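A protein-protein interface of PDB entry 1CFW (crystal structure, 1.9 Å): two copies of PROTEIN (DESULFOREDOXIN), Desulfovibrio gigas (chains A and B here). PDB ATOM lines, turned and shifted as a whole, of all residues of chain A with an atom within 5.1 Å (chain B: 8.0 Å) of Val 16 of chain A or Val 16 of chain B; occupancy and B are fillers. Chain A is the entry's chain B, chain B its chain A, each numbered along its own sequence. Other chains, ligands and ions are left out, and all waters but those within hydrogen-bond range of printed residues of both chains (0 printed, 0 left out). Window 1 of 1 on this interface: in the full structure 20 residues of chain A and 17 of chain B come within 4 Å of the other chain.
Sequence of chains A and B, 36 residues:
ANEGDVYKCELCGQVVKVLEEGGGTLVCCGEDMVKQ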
ATOM      1  N   ASP A   5     -11.264   9.565   4.605  1.00  0.00           N
ATOM      2  CA  ASP A   5     -10.896   8.195   4.229  1.00  0.00           C
ATOM      3  C   ASP A   5      -9.491   7.841   4.701  1.00  0.00           C
ATOM      4  O   ASP A   5      -8.611   8.692   4.629  1.00  0.00           O
ATOM      5  CB  ASP A   5     -10.873   8.075   2.705  1.00  0.00           C
ATOM      6  CG  ASP A   5     -12.307   7.980   2.204  1.00  0.00           C
ATOM      7  OD1 ASP A   5     -13.204   7.962   3.077  1.00  0.00           O
ATOM      8  OD2 ASP A   5     -12.450   7.941   0.968  1.00  0.00           O
ATOM      9  N   VAL A   6      -9.310   6.580   5.037  1.00  0.00           N
ATOM     10  CA  VAL A   6      -8.037   6.012   5.453  1.00  0.00           C
ATOM     11  C   VAL A   6      -7.562   5.004   4.416  1.00  0.00           C
ATOM     12  O   VAL A   6      -8.324   4.110   4.051  1.00  0.00           O
ATOM     13  CB  VAL A   6      -8.132   5.321   6.834  1.00  0.00           C
ATOM     14  CG1 VAL A   6      -6.808   4.666   7.210  1.00  0.00           C
ATOM     15  CG2 VAL A   6      -8.514   6.372   7.871  1.00  0.00           C
ATOM     16  N   TYR A   7      -6.307   5.132   4.005  1.00  0.00           N
ATOM     17  CA  TYR A   7      -5.686   4.277   2.998  1.00  0.00           C
ATOM     18  C   TYR A   7      -4.395   3.646   3.498  1.00  0.00           C
ATOM     19  O   TYR A   7      -3.596   4.264   4.198  1.00  0.00           O
ATOM     20  CB  TYR A   7      -5.389   5.110   1.742  1.00  0.00           C
ATOM     21  CG  TYR A   7      -6.601   5.351   0.878  1.00  0.00           C
ATOM     22  CD1 TYR A   7      -7.421   6.444   1.134  1.00  0.00           C
ATOM     23  CD2 TYR A   7      -6.908   4.501  -0.177  1.00  0.00           C
ATOM     24  CE1 TYR A   7      -8.538   6.670   0.351  1.00  0.00           C
ATOM     25  CE2 TYR A   7      -8.024   4.725  -0.973  1.00  0.00           C
ATOM     26  CZ  TYR A   7      -8.830   5.812  -0.689  1.00  0.00           C
ATOM     27  OH  TYR A   7      -9.932   6.055  -1.478  1.00  0.00           O
ATOM     28  N   GLN A  14       2.587   1.760   5.040  1.00  0.00           N
ATOM     29  CA  GLN A  14       2.306   3.176   5.285  1.00  0.00           C
ATOM     30  C   GLN A  14       0.806   3.459   5.313  1.00  0.00           C
ATOM     31  O   GLN A  14       0.071   2.900   4.491  1.00  0.00           O
ATOM     32  CB  GLN A  14       2.941   4.023   4.165  1.00  0.00           C
ATOM     33  CG  GLN A  14       2.890   5.504   4.493  1.00  0.00           C
ATOM     34  CD  GLN A  14       3.957   6.313   3.783  1.00  0.00           C
ATOM     35  OE1 GLN A  14       4.444   7.280   4.374  1.00  0.00           O
ATOM     36  NE2 GLN A  14       4.332   5.923   2.570  1.00  0.00           N
ATOM     37  N   VAL A  15       0.352   4.314   6.227  1.00  0.00           N
ATOM     38  CA  VAL A  15      -1.079   4.630   6.345  1.00  0.00           C
ATOM     39  C   VAL A  15      -1.326   6.137   6.349  1.00  0.00           C
ATOM     40  O   VAL A  15      -0.720   6.903   7.091  1.00  0.00           O
ATOM     41  CB  VAL A  15      -1.695   4.010   7.616  1.00  0.00           C
ATOM     42  CG1 VAL A  15      -3.183   4.318   7.708  1.00  0.00           C
ATOM     43  CG2 VAL A  15      -1.484   2.494   7.649  1.00  0.00           C
ATOM     44  N   VAL A  16      -2.217   6.579   5.462  1.00  0.00           N
ATOM     45  CA  VAL A  16      -2.515   8.001   5.347  1.00  0.00           C
ATOM     46  C   VAL A  16      -4.016   8.235   5.517  1.00  0.00           C
ATOM     47  O   VAL A  16      -4.781   7.311   5.243  1.00  0.00           O
ATOM     48  CB  VAL A  16      -2.046   8.602   4.008  1.00  0.00           C
ATOM     49  CG1 VAL A  16      -0.553   8.370   3.865  1.00  0.00           C
ATOM     50  CG2 VAL A  16      -2.815   8.016   2.833  1.00  0.00           C
ATOM     51  N   LYS A  17      -4.358   9.429   5.981  1.00  0.00           N
ATOM     52  CA  LYS A  17      -5.728   9.914   6.074  1.00  0.00           C
ATOM     53  C   LYS A  17      -5.933  11.096   5.130  1.00  0.00           C
ATOM     54  O   LYS A  17      -5.088  11.998   5.147  1.00  0.00           O
ATOM     55  CB  LYS A  17      -6.069  10.358   7.502  1.00  0.00           C
ATOM     56  CG  LYS A  17      -7.556  10.662   7.690  1.00  0.00           C
ATOM     57  CD  LYS A  17      -7.852  10.869   9.174  1.00  0.00           C
ATOM     58  CE  LYS A  17      -9.354  10.879   9.425  1.00  0.00           C
ATOM     59  N   VAL A  18      -7.014  11.089   4.361  1.00  0.00           N
ATOM     60  CA  VAL A  18      -7.356  12.152   3.416  1.00  0.00           C
ATOM     61  C   VAL A  18      -7.884  13.387   4.140  1.00  0.00           C
ATOM     62  O   VAL A  18      -8.884  13.273   4.860  1.00  0.00           O
ATOM     63  CB  VAL A  18      -8.356  11.696   2.331  1.00  0.00           C
ATOM     64  CG1 VAL A  18      -8.729  12.829   1.377  1.00  0.00           C
ATOM     65  CG2 VAL A  18      -7.749  10.557   1.516  1.00  0.00           C
ATOM     66  N   LEU A  19      -7.188  14.522   3.967  1.00  0.00           N
ATOM     67  CA  LEU A  19      -7.656  15.752   4.604  1.00  0.00           C
ATOM     68  C   LEU A  19      -8.438  16.646   3.649  1.00  0.00           C
ATOM     69  O   LEU A  19      -9.285  17.411   4.093  1.00  0.00           O
ATOM     70  CB  LEU A  19      -6.516  16.607   5.155  1.00  0.00           C
ATOM     71  CG  LEU A  19      -5.665  15.928   6.235  1.00  0.00           C
ATOM     72  CD1 LEU A  19      -4.474  16.824   6.517  1.00  0.00           C
ATOM     73  CD2 LEU A  19      -6.538  15.667   7.451  1.00  0.00           C
ATOM     74  N   LEU A  26      -4.377   7.524  -5.035  1.00  0.00           N
ATOM     75  CA  LEU A  26      -3.216   7.462  -4.158  1.00  0.00           C
ATOM     76  C   LEU A  26      -2.478   6.142  -4.389  1.00  0.00           C
ATOM     77  O   LEU A  26      -3.076   5.062  -4.407  1.00  0.00           O
ATOM     78  CB  LEU A  26      -3.682   7.547  -2.698  1.00  0.00           C
ATOM     79  CG  LEU A  26      -4.247   8.896  -2.241  1.00  0.00           C
ATOM     80  CD1 LEU A  26      -4.771   8.761  -0.808  1.00  0.00           C
ATOM     81  CD2 LEU A  26      -3.213   9.998  -2.356  1.00  0.00           C
ATOM     82  N   MET A  33      -3.060   2.335  -3.209  1.00  0.00           N
ATOM     83  CA  MET A  33      -3.263   2.149  -1.772  1.00  0.00           C
ATOM     84  C   MET A  33      -4.653   1.592  -1.501  1.00  0.00           C
ATOM     85  O   MET A  33      -5.587   1.845  -2.259  1.00  0.00           O
ATOM     86  CB  MET A  33      -3.053   3.465  -1.016  1.00  0.00           C
ATOM     87  CG  MET A  33      -1.589   3.914  -1.037  1.00  0.00           C
ATOM     88  SD  MET A  33      -1.362   5.451  -0.130  1.00  0.00           S
ATOM     89  CE  MET A  33      -0.913   4.841   1.498  1.00  0.00           C
ATOM     90  N   ALA B   1       7.493   8.072   4.685  1.00  0.00           N
ATOM     91  CA  ALA B   1       7.243   9.421   5.186  1.00  0.00           C
ATOM     92  C   ALA B   1       7.072   9.388   6.701  1.00  0.00           C
ATOM     93  O   ALA B   1       6.758   8.331   7.251  1.00  0.00           O
ATOM     94  CB  ALA B   1       6.027  10.023   4.498  1.00  0.00           C
ATOM     95  N   GLY B   4       2.736  12.175  11.107  1.00  0.00           N
ATOM     96  CA  GLY B   4       2.440  13.578  11.318  1.00  0.00           C
ATOM     97  C   GLY B   4       2.692  14.425  10.084  1.00  0.00           C
ATOM     98  O   GLY B   4       2.103  15.498   9.952  1.00  0.00           O
ATOM     99  N   ASP B   5       3.540  13.977   9.159  1.00  0.00           N
ATOM    100  CA  ASP B   5       3.782  14.757   7.943  1.00  0.00           C
ATOM    101  C   ASP B   5       2.508  14.932   7.124  1.00  0.00           C
ATOM    102  O   ASP B   5       1.621  14.076   7.059  1.00  0.00           O
ATOM    103  CB  ASP B   5       4.786  13.997   7.058  1.00  0.00           C
ATOM    104  CG  ASP B   5       6.185  14.054   7.642  1.00  0.00           C
ATOM    105  OD1 ASP B   5       6.365  14.934   8.511  1.00  0.00           O
ATOM    106  OD2 ASP B   5       7.049  13.249   7.237  1.00  0.00           O
ATOM    107  N   VAL B   6       2.445  16.029   6.381  1.00  0.00           N
ATOM    108  CA  VAL B   6       1.297  16.259   5.491  1.00  0.00           C
ATOM    109  C   VAL B   6       1.840  16.354   4.063  1.00  0.00           C
ATOM    110  O   VAL B   6       2.889  16.988   3.854  1.00  0.00           O
ATOM    111  CB  VAL B   6       0.560  17.540   5.902  1.00  0.00           C
ATOM    112  CG1 VAL B   6      -0.410  18.014   4.839  1.00  0.00           C
ATOM    113  CG2 VAL B   6      -0.176  17.345   7.231  1.00  0.00           C
ATOM    114  N   TYR B   7       1.201  15.648   3.134  1.00  0.00           N
ATOM    115  CA  TYR B   7       1.640  15.609   1.740  1.00  0.00           C
ATOM    116  C   TYR B   7       0.548  16.114   0.801  1.00  0.00           C
ATOM    117  O   TYR B   7      -0.637  15.841   0.989  1.00  0.00           O
ATOM    118  CB  TYR B   7       2.026  14.182   1.317  1.00  0.00           C
ATOM    119  CG  TYR B   7       3.421  13.840   1.778  1.00  0.00           C
ATOM    120  CD1 TYR B   7       3.652  13.403   3.086  1.00  0.00           C
ATOM    121  CD2 TYR B   7       4.485  13.997   0.907  1.00  0.00           C
ATOM    122  CE1 TYR B   7       4.951  13.114   3.479  1.00  0.00           C
ATOM    123  CE2 TYR B   7       5.777  13.711   1.300  1.00  0.00           C
ATOM    124  CZ  TYR B   7       5.994  13.269   2.589  1.00  0.00           C
ATOM    125  OH  TYR B   7       7.285  12.978   2.963  1.00  0.00           O
ATOM    126  N   LYS B   8       0.956  16.823  -0.242  1.00  0.00           N
ATOM    127  CA  LYS B   8      -0.011  17.390  -1.178  1.00  0.00           C
ATOM    128  C   LYS B   8       0.273  16.993  -2.620  1.00  0.00           C
ATOM    129  O   LYS B   8       1.415  17.023  -3.078  1.00  0.00           O
ATOM    130  CB  LYS B   8       0.101  18.915  -1.098  1.00  0.00           C
ATOM    131  CG  LYS B   8      -0.857  19.698  -1.989  1.00  0.00           C
ATOM    132  CD  LYS B   8      -0.646  21.185  -1.717  1.00  0.00           C
ATOM    133  CE  LYS B   8      -0.999  22.022  -2.934  1.00  0.00           C
ATOM    134  NZ  LYS B   8      -1.195  23.457  -2.574  1.00  0.00           N
ATOM    135  N   CYS B   9      -0.804  16.730  -3.351  1.00  0.00           N
ATOM    136  CA  CYS B   9      -0.700  16.597  -4.801  1.00  0.00           C
ATOM    137  C   CYS B   9      -0.861  17.977  -5.454  1.00  0.00           C
ATOM    138  O   CYS B   9      -1.909  18.610  -5.321  1.00  0.00           O
ATOM    139  CB  CYS B   9      -1.793  15.679  -5.353  1.00  0.00           C
ATOM    140  SG  CYS B   9      -1.602  15.396  -7.142  1.00  0.00           S
ATOM    141  N   GLY B  13      -4.787  18.593  -6.008  1.00  0.00           N
ATOM    142  CA  GLY B  13      -5.139  19.258  -4.753  1.00  0.00           C
ATOM    143  C   GLY B  13      -5.344  18.315  -3.585  1.00  0.00           C
ATOM    144  O   GLY B  13      -5.566  18.760  -2.455  1.00  0.00           O
ATOM    145  N   GLN B  14      -5.269  17.005  -3.815  1.00  0.00           N
ATOM    146  CA  GLN B  14      -5.467  16.067  -2.711  1.00  0.00           C
ATOM    147  C   GLN B  14      -4.397  16.235  -1.635  1.00  0.00           C
ATOM    148  O   GLN B  14      -3.222  16.346  -1.978  1.00  0.00           O
ATOM    149  CB  GLN B  14      -5.464  14.636  -3.226  1.00  0.00           C
ATOM    150  CG  GLN B  14      -5.953  13.629  -2.174  1.00  0.00           C
ATOM    151  CD  GLN B  14      -6.503  12.401  -2.884  1.00  0.00           C
ATOM    152  OE1 GLN B  14      -7.539  11.875  -2.491  1.00  0.00           O
ATOM    153  NE2 GLN B  14      -5.872  11.962  -3.960  1.00  0.00           N
ATOM    154  N   VAL B  15      -4.822  16.249  -0.375  1.00  0.00           N
ATOM    155  CA  VAL B  15      -3.971  16.402   0.796  1.00  0.00           C
ATOM    156  C   VAL B  15      -4.161  15.238   1.767  1.00  0.00           C
ATOM    157  O   VAL B  15      -5.295  14.855   2.071  1.00  0.00           O
ATOM    158  CB  VAL B  15      -4.236  17.726   1.535  1.00  0.00           C
ATOM    159  CG1 VAL B  15      -3.297  17.887   2.726  1.00  0.00           C
ATOM    160  CG2 VAL B  15      -4.061  18.920   0.596  1.00  0.00           C
ATOM    161  N   VAL B  16      -3.072  14.623   2.211  1.00  0.00           N
ATOM    162  CA  VAL B  16      -3.183  13.494   3.140  1.00  0.00           C
ATOM    163  C   VAL B  16      -2.207  13.729   4.292  1.00  0.00           C
ATOM    164  O   VAL B  16      -1.193  14.410   4.145  1.00  0.00           O
ATOM    165  CB  VAL B  16      -2.876  12.116   2.544  1.00  0.00           C
ATOM    166  CG1 VAL B  16      -3.729  11.813   1.328  1.00  0.00           C
ATOM    167  CG2 VAL B  16      -1.397  11.976   2.187  1.00  0.00           C
ATOM    168  N   LYS B  17      -2.546  13.134   5.424  1.00  0.00           N
ATOM    169  CA  LYS B  17      -1.672  13.133   6.596  1.00  0.00           C
ATOM    170  C   LYS B  17      -1.235  11.694   6.845  1.00  0.00           C
ATOM    171  O   LYS B  17      -2.004  10.745   6.683  1.00  0.00           O
ATOM    172  CB  LYS B  17      -2.443  13.671   7.797  1.00  0.00           C
ATOM    173  CG  LYS B  17      -1.694  13.664   9.118  1.00  0.00           C
ATOM    174  CD  LYS B  17      -2.683  13.747  10.285  1.00  0.00           C
ATOM    175  CE  LYS B  17      -2.314  14.904  11.205  1.00  0.00           C
ATOM    176  NZ  LYS B  17      -3.182  15.006  12.405  1.00  0.00           N
ATOM    177  N   VAL B  18       0.034  11.532   7.167  1.00  0.00           N
ATOM    178  CA  VAL B  18       0.611  10.210   7.422  1.00  0.00           C
ATOM    179  C   VAL B  18       0.293   9.758   8.840  1.00  0.00           C
ATOM    180  O   VAL B  18       0.705  10.436   9.792  1.00  0.00           O
ATOM    181  CB  VAL B  18       2.142  10.287   7.227  1.00  0.00           C
ATOM    182  CG1 VAL B  18       2.796   8.949   7.539  1.00  0.00           C
ATOM    183  CG2 VAL B  18       2.420  10.696   5.783  1.00  0.00           C
ATOM    184  N   LEU B  19      -0.434   8.653   8.979  1.00  0.00           N
ATOM    185  CA  LEU B  19      -0.766   8.185  10.330  1.00  0.00           C
ATOM    186  C   LEU B  19       0.250   7.157  10.809  1.00  0.00           C
ATOM    187  O   LEU B  19       0.468   6.921  11.996  1.00  0.00           O
ATOM    188  CB  LEU B  19      -2.153   7.522  10.303  1.00  0.00           C
ATOM    189  CG  LEU B  19      -3.348   8.459  10.114  1.00  0.00           C
ATOM    190  CD1 LEU B  19      -4.666   7.713  10.149  1.00  0.00           C
ATOM    191  CD2 LEU B  19      -3.305   9.532  11.197  1.00  0.00           C
ATOM    192  N   GLU B  20       0.834   6.468   9.838  1.00  0.00           N
ATOM    193  CA  GLU B  20       1.824   5.428  10.121  1.00  0.00           C
ATOM    194  C   GLU B  20       2.913   5.492   9.067  1.00  0.00           C
ATOM    195  O   GLU B  20       2.593   5.376   7.879  1.00  0.00           O
ATOM    196  CB  GLU B  20       1.148   4.049  10.011  1.00  0.00           C
ATOM    197  CG  GLU B  20       2.050   2.930  10.516  1.00  0.00           C
ATOM    198  CD  GLU B  20       1.605   2.546  11.920  1.00  0.00           C
ATOM    199  OE1 GLU B  20       0.417   2.189  12.060  1.00  0.00           O
ATOM    200  OE2 GLU B  20       2.426   2.676  12.849  1.00  0.00           O
ATOM    201  N   GLU B  21       4.142   5.733   9.497  1.00  0.00           N
ATOM    202  CA  GLU B  21       5.253   5.890   8.568  1.00  0.00           C
ATOM    203  C   GLU B  21       5.597   4.579   7.879  1.00  0.00           C
ATOM    204  O   GLU B  21       5.544   3.478   8.412  1.00  0.00           O
ATOM    205  CB  GLU B  21       6.468   6.464   9.303  1.00  0.00           C
ATOM    206  CG  GLU B  21       7.528   5.462   9.710  1.00  0.00           C
ATOM    207  CD  GLU B  21       8.561   6.021  10.671  1.00  0.00           C
ATOM    208  OE2 GLU B  21       9.289   5.237  11.318  1.00  0.00           O
ATOM    209  N   GLY B  22       5.883   4.684   6.590  1.00  0.00           N
ATOM    210  CA  GLY B  22       6.364   3.575   5.774  1.00  0.00           C
ATOM    211  C   GLY B  22       7.408   4.188   4.853  1.00  0.00           C
ATOM    212  O   GLY B  22       7.442   5.412   4.646  1.00  0.00           O
ATOM    213  N   LEU B  26       4.844   8.487  -1.672  1.00  0.00           N
ATOM    214  CA  LEU B  26       3.438   8.728  -1.997  1.00  0.00           C
ATOM    215  C   LEU B  26       3.309   9.419  -3.347  1.00  0.00           C
ATOM    216  O   LEU B  26       4.023  10.393  -3.618  1.00  0.00           O
ATOM    217  CB  LEU B  26       2.777   9.540  -0.882  1.00  0.00           C
ATOM    218  CG  LEU B  26       2.724   8.842   0.488  1.00  0.00           C
ATOM    219  CD1 LEU B  26       2.467   9.865   1.587  1.00  0.00           C
ATOM    220  CD2 LEU B  26       1.642   7.776   0.510  1.00  0.00           C
ATOM    221  N   CYS B  28       0.480  10.623  -6.501  1.00  0.00           N
ATOM    222  CA  CYS B  28      -0.878  10.963  -6.901  1.00  0.00           C
ATOM    223  C   CYS B  28      -0.849  11.649  -8.257  1.00  0.00           C
ATOM    224  O   CYS B  28       0.017  12.503  -8.506  1.00  0.00           O
ATOM    225  CB  CYS B  28      -1.506  11.862  -5.844  1.00  0.00           C
ATOM    226  SG  CYS B  28      -3.266  12.212  -6.136  1.00  0.00           S
ATOM    227  N   MET B  33       3.913  13.120  -4.479  1.00  0.00           N
ATOM    228  CA  MET B  33       3.328  14.141  -3.609  1.00  0.00           C
ATOM    229  C   MET B  33       4.394  14.973  -2.919  1.00  0.00           C
ATOM    230  O   MET B  33       5.501  14.530  -2.639  1.00  0.00           O
ATOM    231  CB  MET B  33       2.421  13.431  -2.580  1.00  0.00           C
ATOM    232  CG  MET B  33       1.207  12.825  -3.314  1.00  0.00           C
ATOM    233  SD  MET B  33       0.040  11.994  -2.195  1.00  0.00           S
ATOM    234  CE  MET B  33      -1.117  13.345  -1.949  1.00  0.00           C
ATOM    235  N   VAL B  34       4.056  16.197  -2.550  1.00  0.00           N
ATOM    236  CA  VAL B  34       4.985  17.142  -1.948  1.00  0.00           C
ATOM    237  C   VAL B  34       4.728  17.323  -0.459  1.00  0.00           C
ATOM    238  O   VAL B  34       3.633  17.632   0.019  1.00  0.00           O
ATOM    239  CB  VAL B  34       4.861  18.494  -2.699  1.00  0.00           C
ATOM    240  CG1 VAL B  34       5.728  19.563  -2.065  1.00  0.00           C
ATOM    241  CG2 VAL B  34       5.264  18.311  -4.158  1.00  0.00           C
ATOM    242  N   LYS B  35       5.772  17.133   0.339  1.00  0.00           N
ATOM    243  CA  LYS B  35       5.621  17.320   1.784  1.00  0.00           C
ATOM    244  C   LYS B  35       5.348  18.779   2.111  1.00  0.00           C
ATOM    245  O   LYS B  35       5.974  19.701   1.583  1.00  0.00           O
ATOM    246  CB  LYS B  35       6.902  16.879   2.504  1.00  0.00           C
ATOM    247  CG  LYS B  35       6.854  17.157   4.007  1.00  0.00           C
ATOM    248  CD  LYS B  35       7.951  16.386   4.726  1.00  0.00           C
ATOM    249  CE  LYS B  35       9.114  17.299   5.086  1.00  0.00           C
ATOM    250  NZ  LYS B  35      10.262  16.532   5.658  1.00  0.00           N
ATOM    251  N   GLN B  36       4.392  19.034   2.998  1.00  0.00           N
ATOM    252  CA  GLN B  36       4.002  20.412   3.260  1.00  0.00           C
ATOM    253  C   GLN B  36       4.790  20.968   4.438  1.00  0.00           C
ATOM    254  O   GLN B  36       4.945  22.202   4.524  1.00  0.00           O
ATOM    255  CB  GLN B  36       2.508  20.531   3.538  1.00  0.00           C
ATOM    256  CG  GLN B  36       1.641  20.411   2.302  1.00  0.00           C
ATOM    257  CD  GLN B  36       2.080  21.251   1.126  1.00  0.00           C
ATOM    258  OE1 GLN B  36       1.738  22.423   1.010  1.00  0.00           O
ATOM    259  NE2 GLN B  36       2.801  20.633   0.194  1.00  0.00           N
ATOM    260  OXT GLN B  36       5.257  20.120   5.220  1.00  0.00           O
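Glu 20 of chain B touches Gln 14 of chain A.
Gln 14 of chain A touches Leu 26 of chain B (NE2 to CD2, 3.9 Å).
Val 15 of chain A touches Val 18 of chain B (O to C, 3.5 Å).
CG2 of Val 16 of chain B touches CB of Val 16 of chain A (3.9 Å).
CA of Val 16 of chain A touches O of Lys 17 of chain B, 3.1 Å away.
C of Val 18 of chain A touches O of Val 15 of chain B, 3.6 Å away.
Leu 19 of chain A touches Lys 17 of chain B.
Leu 26 of chain A touches Gln 14 of chain B (CD2 to NE2, 3.7 Å).
CG1 of Val 16 of chain B touches CD1 of Leu 26 of chain A (3.9 Å).
Met 33 of chain B touches Leu 26 of chain A.
The backbone carbonyl oxygen (O) of Glu 20 of chain B is in hydrogen-bond range of the backbone NH (N) of Val 15 of chain A, 3.0 Å away.
The backbone carbonyl oxygen (O) of Lys 17 of chain B sits at hydrogen-bond distance from the backbone NH (N) of Lys 17 of chain A (2.8 Å).
N of Ala 1 of chain B lies within hydrogen-bond range of OE1 of Gln 14 of chain A, at 3.2 Å.
O of Val 15 of chain A sits at hydrogen-bond distance from N of Leu 19 of chain B (2.6 Å).
O of Val 15 of chain B sits at hydrogen-bond distance from N of Leu 19 of chain A (2.7 Å).
O of Gly 22 of chain B is in hydrogen-bond range of N of Ala 1 of chain B (2.7 Å).
N of Cys 9 of chain B lies within hydrogen-bond range of O of Gln 14 of chain B (2.8 Å).
The backbone carbonyl oxygen of Asp 5 of chain B lies within hydrogen-bond range of the backbone NH of Val 18 of chain B (3.0 Å).
The backbone carbonyl oxygen of Asp 5 of chain A lies within hydrogen-bond range of the backbone NH of Val 18 of chain A, 2.9 Å away.
The backbone carbonyl oxygen (O) of Leu 26 of chain B sits at hydrogen-bond distance from the backbone NH (N) of Met 33 of chain B.
O of Val 16 of chain B sits at hydrogen-bond distance from N of Tyr 7 of chain B, 2.9 Å away.
Hydrophobic or aromatic side chains of chain A that line the printed part of chain B: Val 15, Val 16, Leu 19, Leu 26 and Met 33.
Of the 23 printed residues of chain B, 11 touch a printed residue of chain A.
Printed residues of chain B that touch a printed residue of chain A: Ala 1, Gln 14, Val 15, Val 16, Lys 17, Val 18, Leu 19, Glu 20, Gly 22, Leu 26 and Met 33.
Hydrophobic or aromatic side chains of chain B within 4 Å of the printed part of chain A: Ala 1, Val 16, Val 18, Leu 19, Leu 26 and Met 33.
Val 16 of chain A touches just these residues of chain B: Val 16 and Lys 17.
Printed residues of chain A within 4 Å of Val 16 of chain B: Val 16 (3.9 Å), Lys 17 (3.1 Å) and Leu 26 (3.9 Å).
Of the printed residues of chain B, Leu 19 of chain A touches Val 15 (2.7 Å) and Lys 17 (3.96 Å).
Of the printed residues of chain A, Gly 22 of chain B touches Gln 14 (3.5 Å).
Of the printed residues of chain A, Glu 20 of chain B touches Gln 14 (3.4 Å) and Val 15 (3.0 Å).
Of the printed residues of chain B, Val 15 of chain A touches Val 18 (3.5 Å), Leu 19 (2.6 Å) and Glu 20 (3.0 Å).
Asp 5 of chain B touches none of the printed residues of chain A.
Val 6 of chain B touches none of the printed residues of chain A.
The nearest residue of chain B that does not touch Val 16 of chain A is Leu 26 of chain B (4.1 Å).
The nearest printed residue of chain A that does not touch Val 16 of chain B is Val 18 of chain A (4.2 Å).
The nearest printed residue of chain B that does not touch Val 15 of chain A is Lys 17 of chain B (4.1 Å).
Gln 14 of chain A touches Val 18 of chain B, but with the chains exchanged Val 18 of chain A does not touch Gln 14 of chain B (4.2 Å).
Gln 14 of chain A touches Leu 26 of chain B, and with the chains exchanged Leu 26 of chain A touches Gln 14 of chain B.
Val 15 of chain A touches Val 18 of chain B, and with the chains exchanged Val 18 of chain A touches Val 15 of chain B.
Leu 26 of chain A touches Val 16 of chain B, but with the chains exchanged Val 16 of chain A does not touch Leu 26 of chain B (4.1 Å).
Of the 20 pairs that touch across the chains among the printed residues, 14 have their exchanged pair printed and touching as well.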
